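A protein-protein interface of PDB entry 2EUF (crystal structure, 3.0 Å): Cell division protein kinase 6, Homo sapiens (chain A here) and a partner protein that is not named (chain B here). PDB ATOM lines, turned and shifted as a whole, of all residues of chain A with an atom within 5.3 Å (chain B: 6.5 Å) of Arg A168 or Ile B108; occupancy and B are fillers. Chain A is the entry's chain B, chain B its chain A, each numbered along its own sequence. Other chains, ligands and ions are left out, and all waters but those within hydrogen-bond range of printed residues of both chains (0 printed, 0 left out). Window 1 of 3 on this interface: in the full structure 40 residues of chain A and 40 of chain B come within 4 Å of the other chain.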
ATOM      1  N   ILE A  59     -13.885 -19.374   1.170  1.00  0.00           N
ATOM      2  CA  ILE A  59     -13.390 -20.494   0.363  1.00  0.00           C
ATOM      3  C   ILE A  59     -12.909 -19.995  -0.990  1.00  0.00           C
ATOM      4  O   ILE A  59     -11.786 -20.288  -1.412  1.00  0.00           O
ATOM      5  CB  ILE A  59     -14.475 -21.586   0.191  1.00  0.00           C
ATOM      6  CG1 ILE A  59     -14.603 -22.396   1.475  1.00  0.00           C
ATOM      7  CG2 ILE A  59     -14.133 -22.513  -0.966  1.00  0.00           C
ATOM      8  CD1 ILE A  59     -15.586 -23.499   1.411  1.00  0.00           C
ATOM      9  N   ARG A  60     -13.774 -19.223  -1.641  1.00  0.00           N
ATOM     10  CA  ARG A  60     -13.504 -18.616  -2.924  1.00  0.00           C
ATOM     11  C   ARG A  60     -12.218 -17.792  -2.897  1.00  0.00           C
ATOM     12  O   ARG A  60     -11.292 -18.081  -3.631  1.00  0.00           O
ATOM     13  CB  ARG A  60     -14.699 -17.755  -3.303  1.00  0.00           C
ATOM     14  CG  ARG A  60     -14.528 -16.937  -4.559  1.00  0.00           C
ATOM     15  CD  ARG A  60     -15.761 -16.118  -4.908  1.00  0.00           C
ATOM     16  NE  ARG A  60     -16.815 -16.958  -5.470  1.00  0.00           N
ATOM     17  CZ  ARG A  60     -18.097 -16.610  -5.504  1.00  0.00           C
ATOM     18  NH1 ARG A  60     -18.467 -15.431  -4.995  1.00  0.00           N
ATOM     19  NH2 ARG A  60     -19.011 -17.437  -6.029  1.00  0.00           N
ATOM     20  N   ALA A  63      -9.026 -19.639  -2.664  1.00  0.00           N
ATOM     21  CA  ALA A  63      -8.822 -20.504  -3.822  1.00  0.00           C
ATOM     22  C   ALA A  63      -8.155 -19.742  -4.956  1.00  0.00           C
ATOM     23  O   ALA A  63      -7.279 -20.288  -5.639  1.00  0.00           O
ATOM     24  CB  ALA A  63     -10.144 -21.113  -4.271  1.00  0.00           C
ATOM     25  N   VAL A  64      -8.570 -18.483  -5.116  1.00  0.00           N
ATOM     26  CA  VAL A  64      -8.104 -17.587  -6.176  1.00  0.00           C
ATOM     27  C   VAL A  64      -6.672 -17.140  -5.916  1.00  0.00           C
ATOM     28  O   VAL A  64      -5.831 -17.147  -6.817  1.00  0.00           O
ATOM     29  CB  VAL A  64      -8.987 -16.329  -6.260  1.00  0.00           C
ATOM     30  CG1 VAL A  64      -8.417 -15.319  -7.260  1.00  0.00           C
ATOM     31  CG2 VAL A  64     -10.396 -16.701  -6.619  1.00  0.00           C
ATOM     32  N   ARG A 140      -8.730 -14.303 -15.906  1.00  0.00           N
ATOM     33  CA  ARG A 140     -10.182 -14.398 -15.890  1.00  0.00           C
ATOM     34  C   ARG A 140     -10.733 -14.139 -14.495  1.00  0.00           C
ATOM     35  O   ARG A 140     -11.863 -14.525 -14.196  1.00  0.00           O
ATOM     36  CB  ARG A 140     -10.626 -15.770 -16.423  1.00  0.00           C
ATOM     37  CG  ARG A 140     -10.401 -15.959 -17.915  1.00  0.00           C
ATOM     38  CD  ARG A 140     -10.534 -17.382 -18.405  1.00  0.00           C
ATOM     39  NE  ARG A 140     -11.410 -18.206 -17.572  1.00  0.00           N
ATOM     40  CZ  ARG A 140     -12.597 -18.682 -17.953  1.00  0.00           C
ATOM     41  NH1 ARG A 140     -13.076 -18.409 -19.152  1.00  0.00           N
ATOM     42  NH2 ARG A 140     -13.313 -19.431 -17.136  1.00  0.00           N
ATOM     43  N   VAL A 141      -9.935 -13.501 -13.643  1.00  0.00           N
ATOM     44  CA  VAL A 141     -10.397 -13.107 -12.318  1.00  0.00           C
ATOM     45  C   VAL A 141     -10.835 -11.655 -12.364  1.00  0.00           C
ATOM     46  O   VAL A 141     -10.127 -10.811 -12.902  1.00  0.00           O
ATOM     47  CB  VAL A 141      -9.290 -13.224 -11.250  1.00  0.00           C
ATOM     48  CG1 VAL A 141      -9.831 -12.858  -9.858  1.00  0.00           C
ATOM     49  CG2 VAL A 141      -8.656 -14.613 -11.264  1.00  0.00           C
ATOM     50  N   VAL A 142     -12.007 -11.364 -11.819  1.00  0.00           N
ATOM     51  CA  VAL A 142     -12.420  -9.975 -11.637  1.00  0.00           C
ATOM     52  C   VAL A 142     -12.459  -9.708 -10.142  1.00  0.00           C
ATOM     53  O   VAL A 142     -13.056 -10.492  -9.388  1.00  0.00           O
ATOM     54  CB  VAL A 142     -13.786  -9.629 -12.289  1.00  0.00           C
ATOM     55  CG1 VAL A 142     -13.949  -8.126 -12.388  1.00  0.00           C
ATOM     56  CG2 VAL A 142     -13.882 -10.212 -13.666  1.00  0.00           C
ATOM     57  N   ARG A 144     -13.946  -7.534  -7.922  1.00  0.00           N
ATOM     58  CA  ARG A 144     -15.038  -6.602  -8.070  1.00  0.00           C
ATOM     59  C   ARG A 144     -15.296  -5.766  -6.797  1.00  0.00           C
ATOM     60  O   ARG A 144     -16.437  -5.390  -6.501  1.00  0.00           O
ATOM     61  CB  ARG A 144     -16.273  -7.389  -8.508  1.00  0.00           C
ATOM     62  CG  ARG A 144     -15.941  -8.503  -9.511  1.00  0.00           C
ATOM     63  CD  ARG A 144     -17.068  -9.447  -9.827  1.00  0.00           C
ATOM     64  NE  ARG A 144     -17.570 -10.098  -8.624  1.00  0.00           N
ATOM     65  CZ  ARG A 144     -18.634 -10.894  -8.594  1.00  0.00           C
ATOM     66  NH1 ARG A 144     -19.324 -11.157  -9.703  1.00  0.00           N
ATOM     67  NH2 ARG A 144     -19.014 -11.427  -7.445  1.00  0.00           N
ATOM     68  N   LEU A 166     -14.608 -11.068  -2.796  1.00  0.00           N
ATOM     69  CA  LEU A 166     -15.713 -10.811  -3.706  1.00  0.00           C
ATOM     70  C   LEU A 166     -15.235 -11.043  -5.143  1.00  0.00           C
ATOM     71  O   LEU A 166     -15.963 -10.756  -6.108  1.00  0.00           O
ATOM     72  CB  LEU A 166     -16.209  -9.375  -3.531  1.00  0.00           C
ATOM     73  CG  LEU A 166     -17.676  -9.129  -3.172  1.00  0.00           C
ATOM     74  CD1 LEU A 166     -17.959  -9.542  -1.741  1.00  0.00           C
ATOM     75  CD2 LEU A 166     -18.002  -7.663  -3.333  1.00  0.00           C
ATOM     76  N   ALA A 167     -14.005 -11.550  -5.270  1.00  0.00           N
ATOM     77  CA  ALA A 167     -13.381 -11.808  -6.568  1.00  0.00           C
ATOM     78  C   ALA A 167     -13.885 -13.132  -7.030  1.00  0.00           C
ATOM     79  O   ALA A 167     -14.130 -14.018  -6.199  1.00  0.00           O
ATOM     80  CB  ALA A 167     -11.866 -11.866  -6.454  1.00  0.00           C
ATOM     81  N   ARG A 168     -14.042 -13.293  -8.341  1.00  0.00           N
ATOM     82  CA  ARG A 168     -14.360 -14.611  -8.879  1.00  0.00           C
ATOM     83  C   ARG A 168     -13.942 -14.758 -10.331  1.00  0.00           C
ATOM     84  O   ARG A 168     -13.835 -13.763 -11.049  1.00  0.00           O
ATOM     85  CB  ARG A 168     -15.840 -14.985  -8.647  1.00  0.00           C
ATOM     86  CG  ARG A 168     -16.879 -13.995  -9.156  1.00  0.00           C
ATOM     87  CD  ARG A 168     -18.299 -14.295  -8.660  1.00  0.00           C
ATOM     88  NE  ARG A 168     -18.654 -15.714  -8.744  1.00  0.00           N
ATOM     89  CZ  ARG A 168     -19.542 -16.237  -9.593  1.00  0.00           C
ATOM     90  NH1 ARG A 168     -20.206 -15.470 -10.455  1.00  0.00           N
ATOM     91  NH2 ARG A 168     -19.779 -17.544  -9.565  1.00  0.00           N
ATOM     92  N   ILE A 169     -13.690 -16.003 -10.736  1.00  0.00           N
ATOM     93  CA  ILE A 169     -13.361 -16.340 -12.115  1.00  0.00           C
ATOM     94  C   ILE A 169     -14.573 -16.181 -13.000  1.00  0.00           C
ATOM     95  O   ILE A 169     -15.619 -16.741 -12.710  1.00  0.00           O
ATOM     96  CB  ILE A 169     -12.855 -17.757 -12.186  1.00  0.00           C
ATOM     97  CG1 ILE A 169     -11.513 -17.820 -11.459  1.00  0.00           C
ATOM     98  CG2 ILE A 169     -12.755 -18.185 -13.625  1.00  0.00           C
ATOM     99  CD1 ILE A 169     -10.845 -19.151 -11.441  1.00  0.00           C
ATOM    100  N   TYR A 170     -14.435 -15.399 -14.067  1.00  0.00           N
ATOM    101  CA  TYR A 170     -15.565 -15.120 -14.948  1.00  0.00           C
ATOM    102  C   TYR A 170     -15.655 -16.022 -16.142  1.00  0.00           C
ATOM    103  O   TYR A 170     -14.675 -16.212 -16.880  1.00  0.00           O
ATOM    104  CB  TYR A 170     -15.522 -13.706 -15.468  1.00  0.00           C
ATOM    105  CG  TYR A 170     -16.516 -12.810 -14.798  1.00  0.00           C
ATOM    106  CD1 TYR A 170     -16.519 -12.684 -13.409  1.00  0.00           C
ATOM    107  CD2 TYR A 170     -17.442 -12.070 -15.545  1.00  0.00           C
ATOM    108  CE1 TYR A 170     -17.406 -11.854 -12.776  1.00  0.00           C
ATOM    109  CE2 TYR A 170     -18.341 -11.241 -14.919  1.00  0.00           C
ATOM    110  CZ  TYR A 170     -18.323 -11.124 -13.519  1.00  0.00           C
ATOM    111  OH  TYR A 170     -19.216 -10.285 -12.823  1.00  0.00           O
ATOM    112  N   MET A 174     -22.355 -17.174 -17.012  1.00  0.00           N
ATOM    113  CA  MET A 174     -22.475 -17.473 -15.582  1.00  0.00           C
ATOM    114  C   MET A 174     -23.506 -16.566 -14.858  1.00  0.00           C
ATOM    115  O   MET A 174     -23.799 -15.453 -15.297  1.00  0.00           O
ATOM    116  CB  MET A 174     -21.106 -17.447 -14.891  1.00  0.00           C
ATOM    117  CG  MET A 174     -20.711 -16.121 -14.254  1.00  0.00           C
ATOM    118  SD  MET A 174     -19.030 -15.995 -13.569  1.00  0.00           S
ATOM    119  CE  MET A 174     -18.806 -17.622 -12.816  1.00  0.00           C
ATOM    120  N   ALA A 175     -24.066 -17.057 -13.756  1.00  0.00           N
ATOM    121  CA  ALA A 175     -25.009 -16.289 -12.960  1.00  0.00           C
ATOM    122  C   ALA A 175     -24.260 -15.235 -12.151  1.00  0.00           C
ATOM    123  O   ALA A 175     -23.105 -15.458 -11.774  1.00  0.00           O
ATOM    124  CB  ALA A 175     -25.732 -17.203 -12.062  1.00  0.00           C
ATOM    125  N   LEU A 176     -24.913 -14.095 -11.902  1.00  0.00           N
ATOM    126  CA  LEU A 176     -24.326 -12.953 -11.176  1.00  0.00           C
ATOM    127  C   LEU A 176     -25.229 -12.464 -10.046  1.00  0.00           C
ATOM    128  O   LEU A 176     -26.453 -12.386 -10.219  1.00  0.00           O
ATOM    129  CB  LEU A 176     -24.074 -11.777 -12.124  1.00  0.00           C
ATOM    130  CG  LEU A 176     -23.036 -11.920 -13.243  1.00  0.00           C
ATOM    131  CD1 LEU A 176     -22.868 -10.654 -14.087  1.00  0.00           C
ATOM    132  CD2 LEU A 176     -21.690 -12.355 -12.689  1.00  0.00           C
ATOM    133  N   ASP B  69     -24.517 -23.310 -12.570  1.00  0.00           N
ATOM    134  CA  ASP B  69     -23.683 -22.842 -13.685  1.00  0.00           C
ATOM    135  C   ASP B  69     -22.834 -23.988 -14.189  1.00  0.00           C
ATOM    136  O   ASP B  69     -22.400 -24.853 -13.428  1.00  0.00           O
ATOM    137  CB  ASP B  69     -22.778 -21.688 -13.268  1.00  0.00           C
ATOM    138  CG  ASP B  69     -23.507 -20.328 -13.223  1.00  0.00           C
ATOM    139  OD1 ASP B  69     -23.335 -19.553 -12.224  1.00  0.00           O
ATOM    140  OD2 ASP B  69     -24.258 -19.945 -14.154  1.00  0.00           O
ATOM    141  N   VAL B  72     -19.558 -25.652 -12.567  1.00  0.00           N
ATOM    142  CA  VAL B  72     -19.545 -26.255 -11.223  1.00  0.00           C
ATOM    143  C   VAL B  72     -19.107 -27.723 -11.266  1.00  0.00           C
ATOM    144  O   VAL B  72     -18.141 -28.108 -10.619  1.00  0.00           O
ATOM    145  CB  VAL B  72     -20.907 -26.136 -10.488  1.00  0.00           C
ATOM    146  CG1 VAL B  72     -20.842 -26.828  -9.145  1.00  0.00           C
ATOM    147  CG2 VAL B  72     -21.288 -24.683 -10.267  1.00  0.00           C
ATOM    148  N   LEU B  75     -15.401 -28.748 -11.962  1.00  0.00           N
ATOM    149  CA  LEU B  75     -14.617 -28.391 -10.786  1.00  0.00           C
ATOM    150  C   LEU B  75     -14.915 -29.326  -9.616  1.00  0.00           C
ATOM    151  O   LEU B  75     -14.027 -29.635  -8.824  1.00  0.00           O
ATOM    152  CB  LEU B  75     -14.887 -26.934 -10.419  1.00  0.00           C
ATOM    153  CG  LEU B  75     -14.061 -26.141  -9.407  1.00  0.00           C
ATOM    154  CD1 LEU B  75     -14.572 -26.397  -8.022  1.00  0.00           C
ATOM    155  CD2 LEU B  75     -12.586 -26.423  -9.489  1.00  0.00           C
ATOM    156  N   ILE B  79     -11.904 -31.346  -7.921  1.00  0.00           N
ATOM    157  CA  ILE B  79     -11.681 -31.413  -6.486  1.00  0.00           C
ATOM    158  C   ILE B  79     -11.691 -32.862  -6.041  1.00  0.00           C
ATOM    159  O   ILE B  79     -10.762 -33.327  -5.408  1.00  0.00           O
ATOM    160  CB  ILE B  79     -12.746 -30.630  -5.697  1.00  0.00           C
ATOM    161  CG1 ILE B  79     -12.616 -29.110  -5.929  1.00  0.00           C
ATOM    162  CG2 ILE B  79     -12.634 -30.964  -4.201  1.00  0.00           C
ATOM    163  CD1 ILE B  79     -13.684 -28.267  -5.204  1.00  0.00           C
ATOM    164  N   LEU B 103     -20.663 -29.380  -3.086  1.00  0.00           N
ATOM    165  CA  LEU B 103     -20.887 -28.304  -2.134  1.00  0.00           C
ATOM    166  C   LEU B 103     -19.753 -27.294  -2.182  1.00  0.00           C
ATOM    167  O   LEU B 103     -20.007 -26.090  -2.130  1.00  0.00           O
ATOM    168  CB  LEU B 103     -21.067 -28.837  -0.715  1.00  0.00           C
ATOM    169  CG  LEU B 103     -21.137 -27.773   0.379  1.00  0.00           C
ATOM    170  CD1 LEU B 103     -22.325 -26.849   0.224  1.00  0.00           C
ATOM    171  CD2 LEU B 103     -21.164 -28.442   1.712  1.00  0.00           C
ATOM    172  N   ILE B 104     -18.510 -27.777  -2.271  1.00  0.00           N
ATOM    173  CA  ILE B 104     -17.375 -26.861  -2.389  1.00  0.00           C
ATOM    174  C   ILE B 104     -17.402 -26.182  -3.765  1.00  0.00           C
ATOM    175  O   ILE B 104     -17.310 -24.951  -3.861  1.00  0.00           O
ATOM    176  CB  ILE B 104     -15.996 -27.545  -2.079  1.00  0.00           C
ATOM    177  CG1 ILE B 104     -15.921 -27.976  -0.614  1.00  0.00           C
ATOM    178  CG2 ILE B 104     -14.864 -26.572  -2.293  1.00  0.00           C
ATOM    179  CD1 ILE B 104     -14.709 -28.817  -0.254  1.00  0.00           C
ATOM    180  N   GLY B 105     -17.561 -26.977  -4.821  1.00  0.00           N
ATOM    181  CA  GLY B 105     -17.589 -26.437  -6.178  1.00  0.00           C
ATOM    182  C   GLY B 105     -18.636 -25.354  -6.373  1.00  0.00           C
ATOM    183  O   GLY B 105     -18.381 -24.319  -6.989  1.00  0.00           O
ATOM    184  N   SER B 106     -19.824 -25.601  -5.839  1.00  0.00           N
ATOM    185  CA  SER B 106     -20.895 -24.623  -5.927  1.00  0.00           C
ATOM    186  C   SER B 106     -20.508 -23.332  -5.199  1.00  0.00           C
ATOM    187  O   SER B 106     -20.707 -22.248  -5.729  1.00  0.00           O
ATOM    188  CB  SER B 106     -22.198 -25.195  -5.378  1.00  0.00           C
ATOM    189  OG  SER B 106     -21.986 -25.791  -4.109  1.00  0.00           O
ATOM    190  N   LYS B 107     -19.929 -23.461  -4.009  1.00  0.00           N
ATOM    191  CA  LYS B 107     -19.468 -22.302  -3.246  1.00  0.00           C
ATOM    192  C   LYS B 107     -18.523 -21.404  -4.044  1.00  0.00           C
ATOM    193  O   LYS B 107     -18.635 -20.176  -3.970  1.00  0.00           O
ATOM    194  CB  LYS B 107     -18.852 -22.709  -1.903  1.00  0.00           C
ATOM    195  CG  LYS B 107     -19.896 -23.047  -0.865  1.00  0.00           C
ATOM    196  CD  LYS B 107     -19.336 -23.840   0.279  1.00  0.00           C
ATOM    197  CE  LYS B 107     -20.267 -23.710   1.467  1.00  0.00           C
ATOM    198  NZ  LYS B 107     -19.621 -23.958   2.802  1.00  0.00           N
ATOM    199  N   ILE B 108     -17.625 -21.993  -4.827  1.00  0.00           N
ATOM    200  CA  ILE B 108     -16.783 -21.161  -5.682  1.00  0.00           C
ATOM    201  C   ILE B 108     -17.489 -20.698  -6.959  1.00  0.00           C
ATOM    202  O   ILE B 108     -17.725 -19.500  -7.125  1.00  0.00           O
ATOM    203  CB  ILE B 108     -15.436 -21.816  -6.008  1.00  0.00           C
ATOM    204  CG1 ILE B 108     -14.691 -22.123  -4.716  1.00  0.00           C
ATOM    205  CG2 ILE B 108     -14.625 -20.899  -6.932  1.00  0.00           C
ATOM    206  CD1 ILE B 108     -13.858 -23.320  -4.796  1.00  0.00           C
ATOM    207  N   ARG B 109     -17.850 -21.615  -7.844  1.00  0.00           N
ATOM    208  CA  ARG B 109     -18.132 -21.212  -9.210  1.00  0.00           C
ATOM    209  C   ARG B 109     -19.570 -20.776  -9.563  1.00  0.00           C
ATOM    210  O   ARG B 109     -19.855 -20.440 -10.736  1.00  0.00           O
ATOM    211  CB  ARG B 109     -17.620 -22.284 -10.165  1.00  0.00           C
ATOM    212  CG  ARG B 109     -16.085 -22.312 -10.277  1.00  0.00           C
ATOM    213  CD  ARG B 109     -15.476 -21.338 -11.278  1.00  0.00           C
ATOM    214  NE  ARG B 109     -14.093 -21.713 -11.523  1.00  0.00           N
ATOM    215  CZ  ARG B 109     -13.586 -21.999 -12.721  1.00  0.00           C
ATOM    216  NH1 ARG B 109     -14.333 -21.911 -13.809  1.00  0.00           N
ATOM    217  NH2 ARG B 109     -12.312 -22.367 -12.842  1.00  0.00           N
ATOM    218  N   THR B 110     -20.461 -20.746  -8.567  1.00  0.00           N
ATOM    219  CA  THR B 110     -21.867 -20.386  -8.801  1.00  0.00           C
ATOM    220  C   THR B 110     -22.461 -19.472  -7.729  1.00  0.00           C
ATOM    221  O   THR B 110     -22.189 -19.628  -6.530  1.00  0.00           O
ATOM    222  CB  THR B 110     -22.732 -21.645  -8.990  1.00  0.00           C
ATOM    223  OG1 THR B 110     -23.862 -21.330  -9.813  1.00  0.00           O
ATOM    224  CG2 THR B 110     -23.347 -22.130  -7.658  1.00  0.00           C
ATOM    225  N   VAL B 111     -23.285 -18.522  -8.170  1.00  0.00           N
ATOM    226  CA  VAL B 111     -23.828 -17.491  -7.272  1.00  0.00           C
ATOM    227  C   VAL B 111     -24.750 -18.066  -6.190  1.00  0.00           C
ATOM    228  O   VAL B 111     -24.690 -17.636  -5.037  1.00  0.00           O
ATOM    229  CB  VAL B 111     -24.522 -16.338  -8.047  1.00  0.00           C
ATOM    230  CG1 VAL B 111     -25.590 -16.873  -8.971  1.00  0.00           C
ATOM    231  CG2 VAL B 111     -25.109 -15.325  -7.096  1.00  0.00           C
ATOM    232  N   PRO B 113     -25.170 -21.361  -4.324  1.00  0.00           N
ATOM    233  CA  PRO B 113     -24.458 -22.628  -4.126  1.00  0.00           C
ATOM    234  C   PRO B 113     -25.341 -23.630  -3.455  1.00  0.00           C
ATOM    235  O   PRO B 113     -26.270 -23.254  -2.734  1.00  0.00           O
ATOM    236  CB  PRO B 113     -23.303 -22.251  -3.196  1.00  0.00           C
ATOM    237  CG  PRO B 113     -23.775 -21.024  -2.455  1.00  0.00           C
ATOM    238  CD  PRO B 113     -24.914 -20.405  -3.233  1.00  0.00           C
ATOM    239  N   THR B 147      -8.059 -24.838  -4.193  1.00  0.00           N
ATOM    240  CA  THR B 147      -9.285 -25.514  -4.547  1.00  0.00           C
ATOM    241  C   THR B 147      -9.536 -25.443  -6.038  1.00  0.00           C
ATOM    242  O   THR B 147      -9.891 -26.428  -6.668  1.00  0.00           O
ATOM    243  CB  THR B 147     -10.419 -24.824  -3.805  1.00  0.00           C
ATOM    244  OG1 THR B 147     -10.184 -24.899  -2.398  1.00  0.00           O
ATOM    245  CG2 THR B 147     -11.640 -25.592  -3.927  1.00  0.00           C
ATOM    246  N   GLU B 148      -9.352 -24.251  -6.587  1.00  0.00           N
ATOM    247  CA  GLU B 148      -9.616 -23.933  -7.985  1.00  0.00           C
ATOM    248  C   GLU B 148      -8.775 -24.810  -8.940  1.00  0.00           C
ATOM    249  O   GLU B 148      -7.977 -25.639  -8.500  1.00  0.00           O
ATOM    250  CB  GLU B 148      -9.342 -22.438  -8.153  1.00  0.00           C
ATOM    251  CG  GLU B 148      -9.974 -21.718  -9.325  1.00  0.00           C
ATOM    252  CD  GLU B 148     -11.405 -22.113  -9.606  1.00  0.00           C
ATOM    253  OE1 GLU B 148     -11.573 -23.192 -10.214  1.00  0.00           O
ATOM    254  OE2 GLU B 148     -12.346 -21.335  -9.283  1.00  0.00           O
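The side-chain carboxylate (OD2) of Asp B69 lies within hydrogen-bond range of the backbone NH (N) of Ala A175.
NH2 of Arg A168 sits close to N of Thr B110, 3.4 Å away.
The backbone carbonyl oxygen (O) of Lys B107 lies within hydrogen-bond range of the guanidinium group (NH2) of Arg A60 (3.4 Å).
The backbone carbonyl oxygen (O) of Arg B109 lies within hydrogen-bond range of the guanidinium group (NH2) of Arg A168, at 3.1 Å.
The backbone carbonyl oxygen (O) of Ile B108 is in hydrogen-bond range of the guanidinium group (NH2) of Arg A60 (2.7 Å).
SD of Met A174 is in hydrogen-bond range of NH1 of Arg A168 (3.4 Å).
O of Arg A168 sits at hydrogen-bond distance from N of Val A142, at 3.1 Å.
NH1 of Arg A168 lies within hydrogen-bond range of O of Ala A175, 3.2 Å away.
OD1 of Asp B69 sits at hydrogen-bond distance from OG1 of Thr B110 (3.0 Å).
OE1 of Glu B148 lies within salt-bridge range of NH2 of Arg B109.
Ile A59 touches Lys B107 (CD1 to CD, 3.9 Å).
Ile B108 touches Ile A59 (CG1 to CG2, 3.8 Å).
Ala A63 touches Thr B147.
CB of Glu B148 touches O of Ala A63, 3.9 Å away.
Arg A168 touches Ile B108.
Arg A168 touches Val B111 (NH2 to N, 3.9 Å).
Ile A169 touches Arg B109 (CD1 to NH2, 3.8 Å).
Ile A169 touches Glu B148.
Met A174 touches Asp B69.
Arg B109 touches Met A174 (O to CE, 3.7 Å).
Of the printed residues of chain B, Ile A59 touches Lys B107 (3.9 Å) and Ile B108 (3.8 Å).
Of the printed residues of chain B, Arg A60 touches Lys B107, Ile B108 and Thr B110.
Of chain B, only Ile B108, Arg B109, Thr B110 and Val B111 come within 4 Å of Arg A168.
Of the printed residues of chain A, Asp B69 touches Met A174 (3.4 Å) and Ala A175 (2.9 Å).
Ser B106 touches none of the printed residues of chain A.
Printed residues of chain A within 4 Å of Thr B110: Arg A60 (3.9 Å) and Arg A168 (3.4 Å).
Printed residues of chain A within 4 Å of Val B111: Arg A168 (3.9 Å) and Ala A175 (3.1 Å).
Of the 16 printed residues of chain B, 8 touch a printed residue of chain A.
Printed residues of chain B that touch a printed residue of chain A: Asp B69, Lys B107, Ile B108, Arg B109, Thr B110, Val B111, Thr B147 and Glu B148.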
